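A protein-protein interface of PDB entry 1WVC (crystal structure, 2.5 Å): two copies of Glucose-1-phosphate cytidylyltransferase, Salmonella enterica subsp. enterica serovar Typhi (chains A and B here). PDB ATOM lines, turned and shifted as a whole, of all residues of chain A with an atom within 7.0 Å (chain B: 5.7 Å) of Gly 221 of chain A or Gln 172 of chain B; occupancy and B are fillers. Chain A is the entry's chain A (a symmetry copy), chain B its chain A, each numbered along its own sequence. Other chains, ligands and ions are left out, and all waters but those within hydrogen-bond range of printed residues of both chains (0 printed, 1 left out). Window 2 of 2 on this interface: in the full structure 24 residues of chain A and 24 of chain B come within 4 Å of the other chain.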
ATOM      1  N   PHE A 144       9.461   6.333   0.308  1.00  0.00           N
ATOM      2  CA  PHE A 144       9.675   5.900  -1.042  1.00  0.00           C
ATOM      3  C   PHE A 144       8.322   5.820  -1.724  1.00  0.00           C
ATOM      4  O   PHE A 144       8.137   6.279  -2.852  1.00  0.00           O
ATOM      5  CB  PHE A 144      10.284   4.502  -0.936  1.00  0.00           C
ATOM      6  CG  PHE A 144      10.243   3.746  -2.224  1.00  0.00           C
ATOM      7  CD1 PHE A 144      11.357   3.740  -3.056  1.00  0.00           C
ATOM      8  CD2 PHE A 144       9.108   3.032  -2.611  1.00  0.00           C
ATOM      9  CE1 PHE A 144      11.338   3.033  -4.255  1.00  0.00           C
ATOM     10  CE2 PHE A 144       9.070   2.327  -3.813  1.00  0.00           C
ATOM     11  CZ  PHE A 144      10.196   2.330  -4.635  1.00  0.00           C
ATOM     12  N   LYS A 150       2.703   6.457  -6.374  1.00  0.00           N
ATOM     13  CA  LYS A 150       1.828   5.418  -6.936  1.00  0.00           C
ATOM     14  C   LYS A 150       1.028   4.760  -5.835  1.00  0.00           C
ATOM     15  O   LYS A 150       1.398   4.912  -4.650  1.00  0.00           O
ATOM     16  CB  LYS A 150       2.530   4.365  -7.794  1.00  0.00           C
ATOM     17  CG  LYS A 150       3.665   4.933  -8.636  1.00  0.00           C
ATOM     18  CD  LYS A 150       3.556   4.612 -10.122  1.00  0.00           C
ATOM     19  CE  LYS A 150       4.144   5.710 -11.006  1.00  0.00           C
ATOM     20  NZ  LYS A 150       3.629   5.682 -12.389  1.00  0.00           N
ATOM     21  N   LYS A 151      -0.059   4.083  -6.205  1.00  0.00           N
ATOM     22  CA  LYS A 151      -0.943   3.411  -5.250  1.00  0.00           C
ATOM     23  C   LYS A 151      -0.316   2.369  -4.320  1.00  0.00           C
ATOM     24  O   LYS A 151      -0.698   2.283  -3.152  1.00  0.00           O
ATOM     25  CB  LYS A 151      -2.192   2.825  -5.893  1.00  0.00           C
ATOM     26  CG  LYS A 151      -2.597   3.469  -7.207  1.00  0.00           C
ATOM     27  CD  LYS A 151      -4.049   3.134  -7.554  1.00  0.00           C
ATOM     28  CE  LYS A 151      -4.222   1.998  -8.561  1.00  0.00           C
ATOM     29  NZ  LYS A 151      -5.630   1.779  -8.985  1.00  0.00           N
ATOM     30  N   MET A 215      -1.249  -8.127  -9.480  1.00  0.00           N
ATOM     31  CA  MET A 215      -0.928  -8.248 -10.911  1.00  0.00           C
ATOM     32  C   MET A 215      -1.412  -7.025 -11.688  1.00  0.00           C
ATOM     33  O   MET A 215      -0.644  -6.405 -12.448  1.00  0.00           O
ATOM     34  CB  MET A 215      -1.560  -9.518 -11.487  1.00  0.00           C
ATOM     35  CG  MET A 215      -0.834 -10.773 -11.009  1.00  0.00           C
ATOM     36  SD  MET A 215      -1.844 -12.238 -10.957  1.00  0.00           S
ATOM     37  CE  MET A 215      -0.826 -13.559 -11.590  1.00  0.00           C
ATOM     38  N   THR A 216      -2.647  -6.704 -11.480  1.00  0.00           N
ATOM     39  CA  THR A 216      -3.270  -5.577 -12.115  1.00  0.00           C
ATOM     40  C   THR A 216      -2.504  -4.307 -11.809  1.00  0.00           C
ATOM     41  O   THR A 216      -2.283  -3.487 -12.680  1.00  0.00           O
ATOM     42  CB  THR A 216      -4.773  -5.476 -11.748  1.00  0.00           C
ATOM     43  OG1 THR A 216      -5.431  -6.748 -11.810  1.00  0.00           O
ATOM     44  CG2 THR A 216      -5.453  -4.477 -12.676  1.00  0.00           C
ATOM     45  N   LEU A 217      -2.078  -4.154 -10.563  1.00  0.00           N
ATOM     46  CA  LEU A 217      -1.332  -2.969 -10.156  1.00  0.00           C
ATOM     47  C   LEU A 217      -0.046  -2.832 -10.899  1.00  0.00           C
ATOM     48  O   LEU A 217       0.363  -1.730 -11.279  1.00  0.00           O
ATOM     49  CB  LEU A 217      -1.025  -2.977  -8.651  1.00  0.00           C
ATOM     50  CG  LEU A 217      -2.253  -2.580  -7.855  1.00  0.00           C
ATOM     51  CD1 LEU A 217      -2.250  -3.262  -6.496  1.00  0.00           C
ATOM     52  CD2 LEU A 217      -2.317  -1.062  -7.741  1.00  0.00           C
ATOM     53  N   ALA A 218       0.587  -3.983 -11.075  1.00  0.00           N
ATOM     54  CA  ALA A 218       1.838  -4.026 -11.778  1.00  0.00           C
ATOM     55  C   ALA A 218       1.543  -3.635 -13.208  1.00  0.00           C
ATOM     56  O   ALA A 218       2.111  -2.700 -13.760  1.00  0.00           O
ATOM     57  CB  ALA A 218       2.456  -5.417 -11.691  1.00  0.00           C
ATOM     58  N   GLN A 219       0.614  -4.373 -13.791  1.00  0.00           N
ATOM     59  CA  GLN A 219       0.200  -4.146 -15.157  1.00  0.00           C
ATOM     60  C   GLN A 219      -0.232  -2.710 -15.379  1.00  0.00           C
ATOM     61  O   GLN A 219      -0.104  -2.145 -16.457  1.00  0.00           O
ATOM     62  CB  GLN A 219      -0.981  -5.071 -15.487  1.00  0.00           C
ATOM     63  CG  GLN A 219      -1.520  -4.893 -16.915  1.00  0.00           C
ATOM     64  CD  GLN A 219      -0.525  -5.382 -17.951  1.00  0.00           C
ATOM     65  OE1 GLN A 219      -0.490  -4.900 -19.095  1.00  0.00           O
ATOM     66  NE2 GLN A 219       0.306  -6.335 -17.537  1.00  0.00           N
ATOM     67  N   GLN A 220      -0.765  -2.146 -14.317  1.00  0.00           N
ATOM     68  CA  GLN A 220      -1.272  -0.797 -14.285  1.00  0.00           C
ATOM     69  C   GLN A 220      -0.180   0.232 -14.147  1.00  0.00           C
ATOM     70  O   GLN A 220      -0.441   1.435 -14.110  1.00  0.00           O
ATOM     71  CB  GLN A 220      -2.178  -0.663 -13.050  1.00  0.00           C
ATOM     72  CG  GLN A 220      -3.670  -0.443 -13.363  1.00  0.00           C
ATOM     73  CD  GLN A 220      -4.365   0.335 -12.261  1.00  0.00           C
ATOM     74  OE1 GLN A 220      -3.714   1.065 -11.488  1.00  0.00           O
ATOM     75  NE2 GLN A 220      -5.687   0.189 -12.190  1.00  0.00           N
ATOM     76  N   GLY A 221       1.046  -0.226 -14.036  1.00  0.00           N
ATOM     77  CA  GLY A 221       2.125   0.727 -13.885  1.00  0.00           C
ATOM     78  C   GLY A 221       1.991   1.451 -12.561  1.00  0.00           C
ATOM     79  O   GLY A 221       2.595   2.511 -12.330  1.00  0.00           O
ATOM     80  N   GLU A 222       1.174   0.834 -11.705  1.00  0.00           N
ATOM     81  CA  GLU A 222       0.900   1.335 -10.377  1.00  0.00           C
ATOM     82  C   GLU A 222       1.647   0.522  -9.324  1.00  0.00           C
ATOM     83  O   GLU A 222       1.449   0.722  -8.128  1.00  0.00           O
ATOM     84  CB  GLU A 222      -0.605   1.363 -10.046  1.00  0.00           C
ATOM     85  CG  GLU A 222      -1.408   2.473 -10.750  1.00  0.00           C
ATOM     86  CD  GLU A 222      -0.773   3.828 -10.661  1.00  0.00           C
ATOM     87  OE1 GLU A 222      -0.793   4.513  -9.649  1.00  0.00           O
ATOM     88  OE2 GLU A 222      -0.197   4.184 -11.792  1.00  0.00           O
ATOM     89  N   LEU A 223       2.514  -0.402  -9.749  1.00  0.00           N
ATOM     90  CA  LEU A 223       3.244  -1.189  -8.769  1.00  0.00           C
ATOM     91  C   LEU A 223       4.743  -0.921  -8.673  1.00  0.00           C
ATOM     92  O   LEU A 223       5.505  -1.207  -9.594  1.00  0.00           O
ATOM     93  CB  LEU A 223       2.964  -2.686  -8.842  1.00  0.00           C
ATOM     94  CG  LEU A 223       3.675  -3.415  -7.701  1.00  0.00           C
ATOM     95  CD1 LEU A 223       3.260  -2.834  -6.352  1.00  0.00           C
ATOM     96  CD2 LEU A 223       3.386  -4.911  -7.748  1.00  0.00           C
ATOM     97  N   MET A 224       5.149  -0.392  -7.521  1.00  0.00           N
ATOM     98  CA  MET A 224       6.535  -0.064  -7.226  1.00  0.00           C
ATOM     99  C   MET A 224       7.220  -1.095  -6.367  1.00  0.00           C
ATOM    100  O   MET A 224       6.614  -1.779  -5.570  1.00  0.00           O
ATOM    101  CB  MET A 224       6.612   1.272  -6.468  1.00  0.00           C
ATOM    102  CG  MET A 224       6.342   2.405  -7.415  1.00  0.00           C
ATOM    103  SD  MET A 224       6.921   1.960  -9.068  1.00  0.00           S
ATOM    104  CE  MET A 224       8.091   3.302  -9.375  1.00  0.00           C
ATOM    105  N   ALA A 225       8.523  -1.193  -6.503  1.00  0.00           N
ATOM    106  CA  ALA A 225       9.214  -2.156  -5.686  1.00  0.00           C
ATOM    107  C   ALA A 225      10.338  -1.550  -4.877  1.00  0.00           C
ATOM    108  O   ALA A 225      11.296  -0.958  -5.392  1.00  0.00           O
ATOM    109  CB  ALA A 225       9.690  -3.356  -6.484  1.00  0.00           C
ATOM    110  N   GLU A 227      13.436  -2.144  -2.909  1.00  0.00           N
ATOM    111  CA  GLU A 227      14.490  -3.161  -2.822  1.00  0.00           C
ATOM    112  C   GLU A 227      15.191  -3.290  -1.481  1.00  0.00           C
ATOM    113  O   GLU A 227      15.810  -2.354  -0.980  1.00  0.00           O
ATOM    114  CB  GLU A 227      15.564  -3.078  -3.926  1.00  0.00           C
ATOM    115  CG  GLU A 227      15.058  -2.854  -5.369  1.00  0.00           C
ATOM    116  CD  GLU A 227      16.182  -2.863  -6.389  1.00  0.00           C
ATOM    117  OE1 GLU A 227      17.311  -3.278  -6.144  1.00  0.00           O
ATOM    118  OE2 GLU A 227      15.825  -2.366  -7.554  1.00  0.00           O
ATOM    119  N   ASP B 167       9.851  -8.960 -11.911  1.00  0.00           N
ATOM    120  CA  ASP B 167      10.356  -8.213 -13.036  1.00  0.00           C
ATOM    121  C   ASP B 167      10.390  -6.767 -12.587  1.00  0.00           C
ATOM    122  O   ASP B 167       9.352  -6.078 -12.593  1.00  0.00           O
ATOM    123  CB  ASP B 167       9.448  -8.327 -14.268  1.00  0.00           C
ATOM    124  CG  ASP B 167      10.045  -7.623 -15.452  1.00  0.00           C
ATOM    125  OD1 ASP B 167      11.222  -7.306 -15.506  1.00  0.00           O
ATOM    126  OD2 ASP B 167       9.167  -7.387 -16.394  1.00  0.00           O
ATOM    127  N   ILE B 168      11.587  -6.350 -12.166  1.00  0.00           N
ATOM    128  CA  ILE B 168      11.791  -5.006 -11.681  1.00  0.00           C
ATOM    129  C   ILE B 168      12.817  -4.270 -12.471  1.00  0.00           C
ATOM    130  O   ILE B 168      13.974  -4.700 -12.565  1.00  0.00           O
ATOM    131  CB  ILE B 168      12.217  -4.874 -10.222  1.00  0.00           C
ATOM    132  CG1 ILE B 168      11.730  -6.003  -9.328  1.00  0.00           C
ATOM    133  CG2 ILE B 168      11.813  -3.515  -9.653  1.00  0.00           C
ATOM    134  CD1 ILE B 168      12.431  -5.925  -7.982  1.00  0.00           C
ATOM    135  N   GLN B 169      12.328  -3.148 -12.991  1.00  0.00           N
ATOM    136  CA  GLN B 169      13.074  -2.201 -13.793  1.00  0.00           C
ATOM    137  C   GLN B 169      12.842  -0.794 -13.265  1.00  0.00           C
ATOM    138  O   GLN B 169      11.704  -0.348 -13.159  1.00  0.00           O
ATOM    139  CB  GLN B 169      12.697  -2.300 -15.287  1.00  0.00           C
ATOM    140  CG  GLN B 169      13.801  -2.989 -16.116  1.00  0.00           C
ATOM    141  CD  GLN B 169      13.254  -3.919 -17.179  1.00  0.00           C
ATOM    142  OE1 GLN B 169      12.540  -3.495 -18.103  1.00  0.00           O
ATOM    143  NE2 GLN B 169      13.601  -5.196 -17.055  1.00  0.00           N
ATOM    144  N   ALA B 170      13.924  -0.106 -12.919  1.00  0.00           N
ATOM    145  CA  ALA B 170      13.831   1.247 -12.407  1.00  0.00           C
ATOM    146  C   ALA B 170      12.860   1.412 -11.228  1.00  0.00           C
ATOM    147  O   ALA B 170      12.082   2.375 -11.174  1.00  0.00           O
ATOM    148  CB  ALA B 170      13.541   2.215 -13.544  1.00  0.00           C
ATOM    149  N   GLY B 171      12.938   0.458 -10.284  1.00  0.00           N
ATOM    150  CA  GLY B 171      12.134   0.401  -9.059  1.00  0.00           C
ATOM    151  C   GLY B 171      10.656   0.125  -9.285  1.00  0.00           C
ATOM    152  O   GLY B 171       9.826   0.253  -8.380  1.00  0.00           O
ATOM    153  N   GLN B 172      10.345  -0.258 -10.512  1.00  0.00           N
ATOM    154  CA  GLN B 172       8.989  -0.540 -10.889  1.00  0.00           C
ATOM    155  C   GLN B 172       8.770  -2.002 -11.207  1.00  0.00           C
ATOM    156  O   GLN B 172       9.439  -2.591 -12.065  1.00  0.00           O
ATOM    157  CB  GLN B 172       8.568   0.353 -12.076  1.00  0.00           C
ATOM    158  CG  GLN B 172       7.231  -0.053 -12.722  1.00  0.00           C
ATOM    159  CD  GLN B 172       6.503   1.125 -13.348  1.00  0.00           C
ATOM    160  OE1 GLN B 172       5.531   0.955 -14.091  1.00  0.00           O
ATOM    161  NE2 GLN B 172       6.968   2.336 -13.046  1.00  0.00           N
ATOM    162  N   VAL B 173       7.813  -2.583 -10.498  1.00  0.00           N
ATOM    163  CA  VAL B 173       7.506  -3.968 -10.732  1.00  0.00           C
ATOM    164  C   VAL B 173       6.774  -4.062 -12.036  1.00  0.00           C
ATOM    165  O   VAL B 173       5.654  -3.559 -12.154  1.00  0.00           O
ATOM    166  CB  VAL B 173       6.661  -4.578  -9.626  1.00  0.00           C
ATOM    167  CG1 VAL B 173       6.489  -6.085  -9.887  1.00  0.00           C
ATOM    168  CG2 VAL B 173       7.328  -4.279  -8.277  1.00  0.00           C
ATOM    169  N   ARG B 174       7.420  -4.685 -13.009  1.00  0.00           N
ATOM    170  CA  ARG B 174       6.802  -4.820 -14.319  1.00  0.00           C
ATOM    171  C   ARG B 174       5.852  -6.004 -14.372  1.00  0.00           C
ATOM    172  O   ARG B 174       4.792  -5.962 -15.024  1.00  0.00           O
ATOM    173  CB  ARG B 174       7.812  -4.839 -15.474  1.00  0.00           C
ATOM    174  CG  ARG B 174       7.589  -3.707 -16.479  1.00  0.00           C
ATOM    175  CD  ARG B 174       8.732  -3.513 -17.481  1.00  0.00           C
ATOM    176  NE  ARG B 174       8.380  -3.798 -18.889  1.00  0.00           N
ATOM    177  CZ  ARG B 174       9.161  -3.515 -19.956  1.00  0.00           C
ATOM    178  NH1 ARG B 174      10.359  -2.940 -19.798  1.00  0.00           N
ATOM    179  NH2 ARG B 174       8.749  -3.815 -21.209  1.00  0.00           N
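SD of Met 224 of chain A sits close to O of Gly 171 of chain B (3.4 Å).
O of Gly 171 of chain B sits at hydrogen-bond distance from N of Ala 225 of chain A.
The backbone carbonyl oxygen (O) of Leu 223 of chain A lies within hydrogen-bond range of the backbone NH (N) of Val 173 of chain B (2.8 Å).
The backbone NH (N) of Leu 223 of chain A is in hydrogen-bond range of the backbone carbonyl oxygen (O) of Leu 217 of chain A.
O of Gly 221 of chain A lies close to NZ of Lys 150 of chain A, at 3.3 Å.
Among the printed residues, merely in contact across the chains: Ala 225 of chain A with Val 173 of chain B, Gly 221 of chain A with Gln 172 of chain B, Met 224 of chain A with Val 173 of chain B, Met 224 of chain A with Gln 172 of chain B, Ala 218 of chain A with Val 173 of chain B, Leu 223 of chain A with Gln 172 of chain B and Ala 225 of chain A with Ile 168 of chain B.
Of the printed residues of chain B, Ala 218 of chain A touches Val 173 (3.7 Å).
Gly 221 of chain A touches just one residue of chain B: Gln 172.
Printed residues of chain B within 4 Å of Met 224 of chain A: Gly 171, Gln 172 and Val 173.
Printed residues of chain A within 4 Å of Ile 168 of chain B: Ala 225 (3.8 Å).
Gln 169 of chain B touches none of the printed residues of chain A.
Printed residues of chain A within 4 Å of Gln 172 of chain B: Gly 221, Leu 223 and Met 224.
Of the printed residues of chain A, Val 173 of chain B touches Ala 218 (3.7 Å), Leu 223 (2.8 Å), Met 224 (3.7 Å) and Ala 225 (3.1 Å).
The nearest residue of chain A that does not touch Gln 172 of chain B is Ala 225 of chain A (4.5 Å).
Of the 15 printed residues of chain A, 5 touch a printed residue of chain B.
Hydrophobic or aromatic side chains of chain A that line the printed part of chain B: Ala 218, Leu 223, Met 224 and Ala 225.
Printed residues of chain B that touch a printed residue of chain A: Ile 168, Gly 171, Gln 172 and Val 173.
Among the printed residues, 10 pairs touch across the chains.
No position is printed for both chains.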
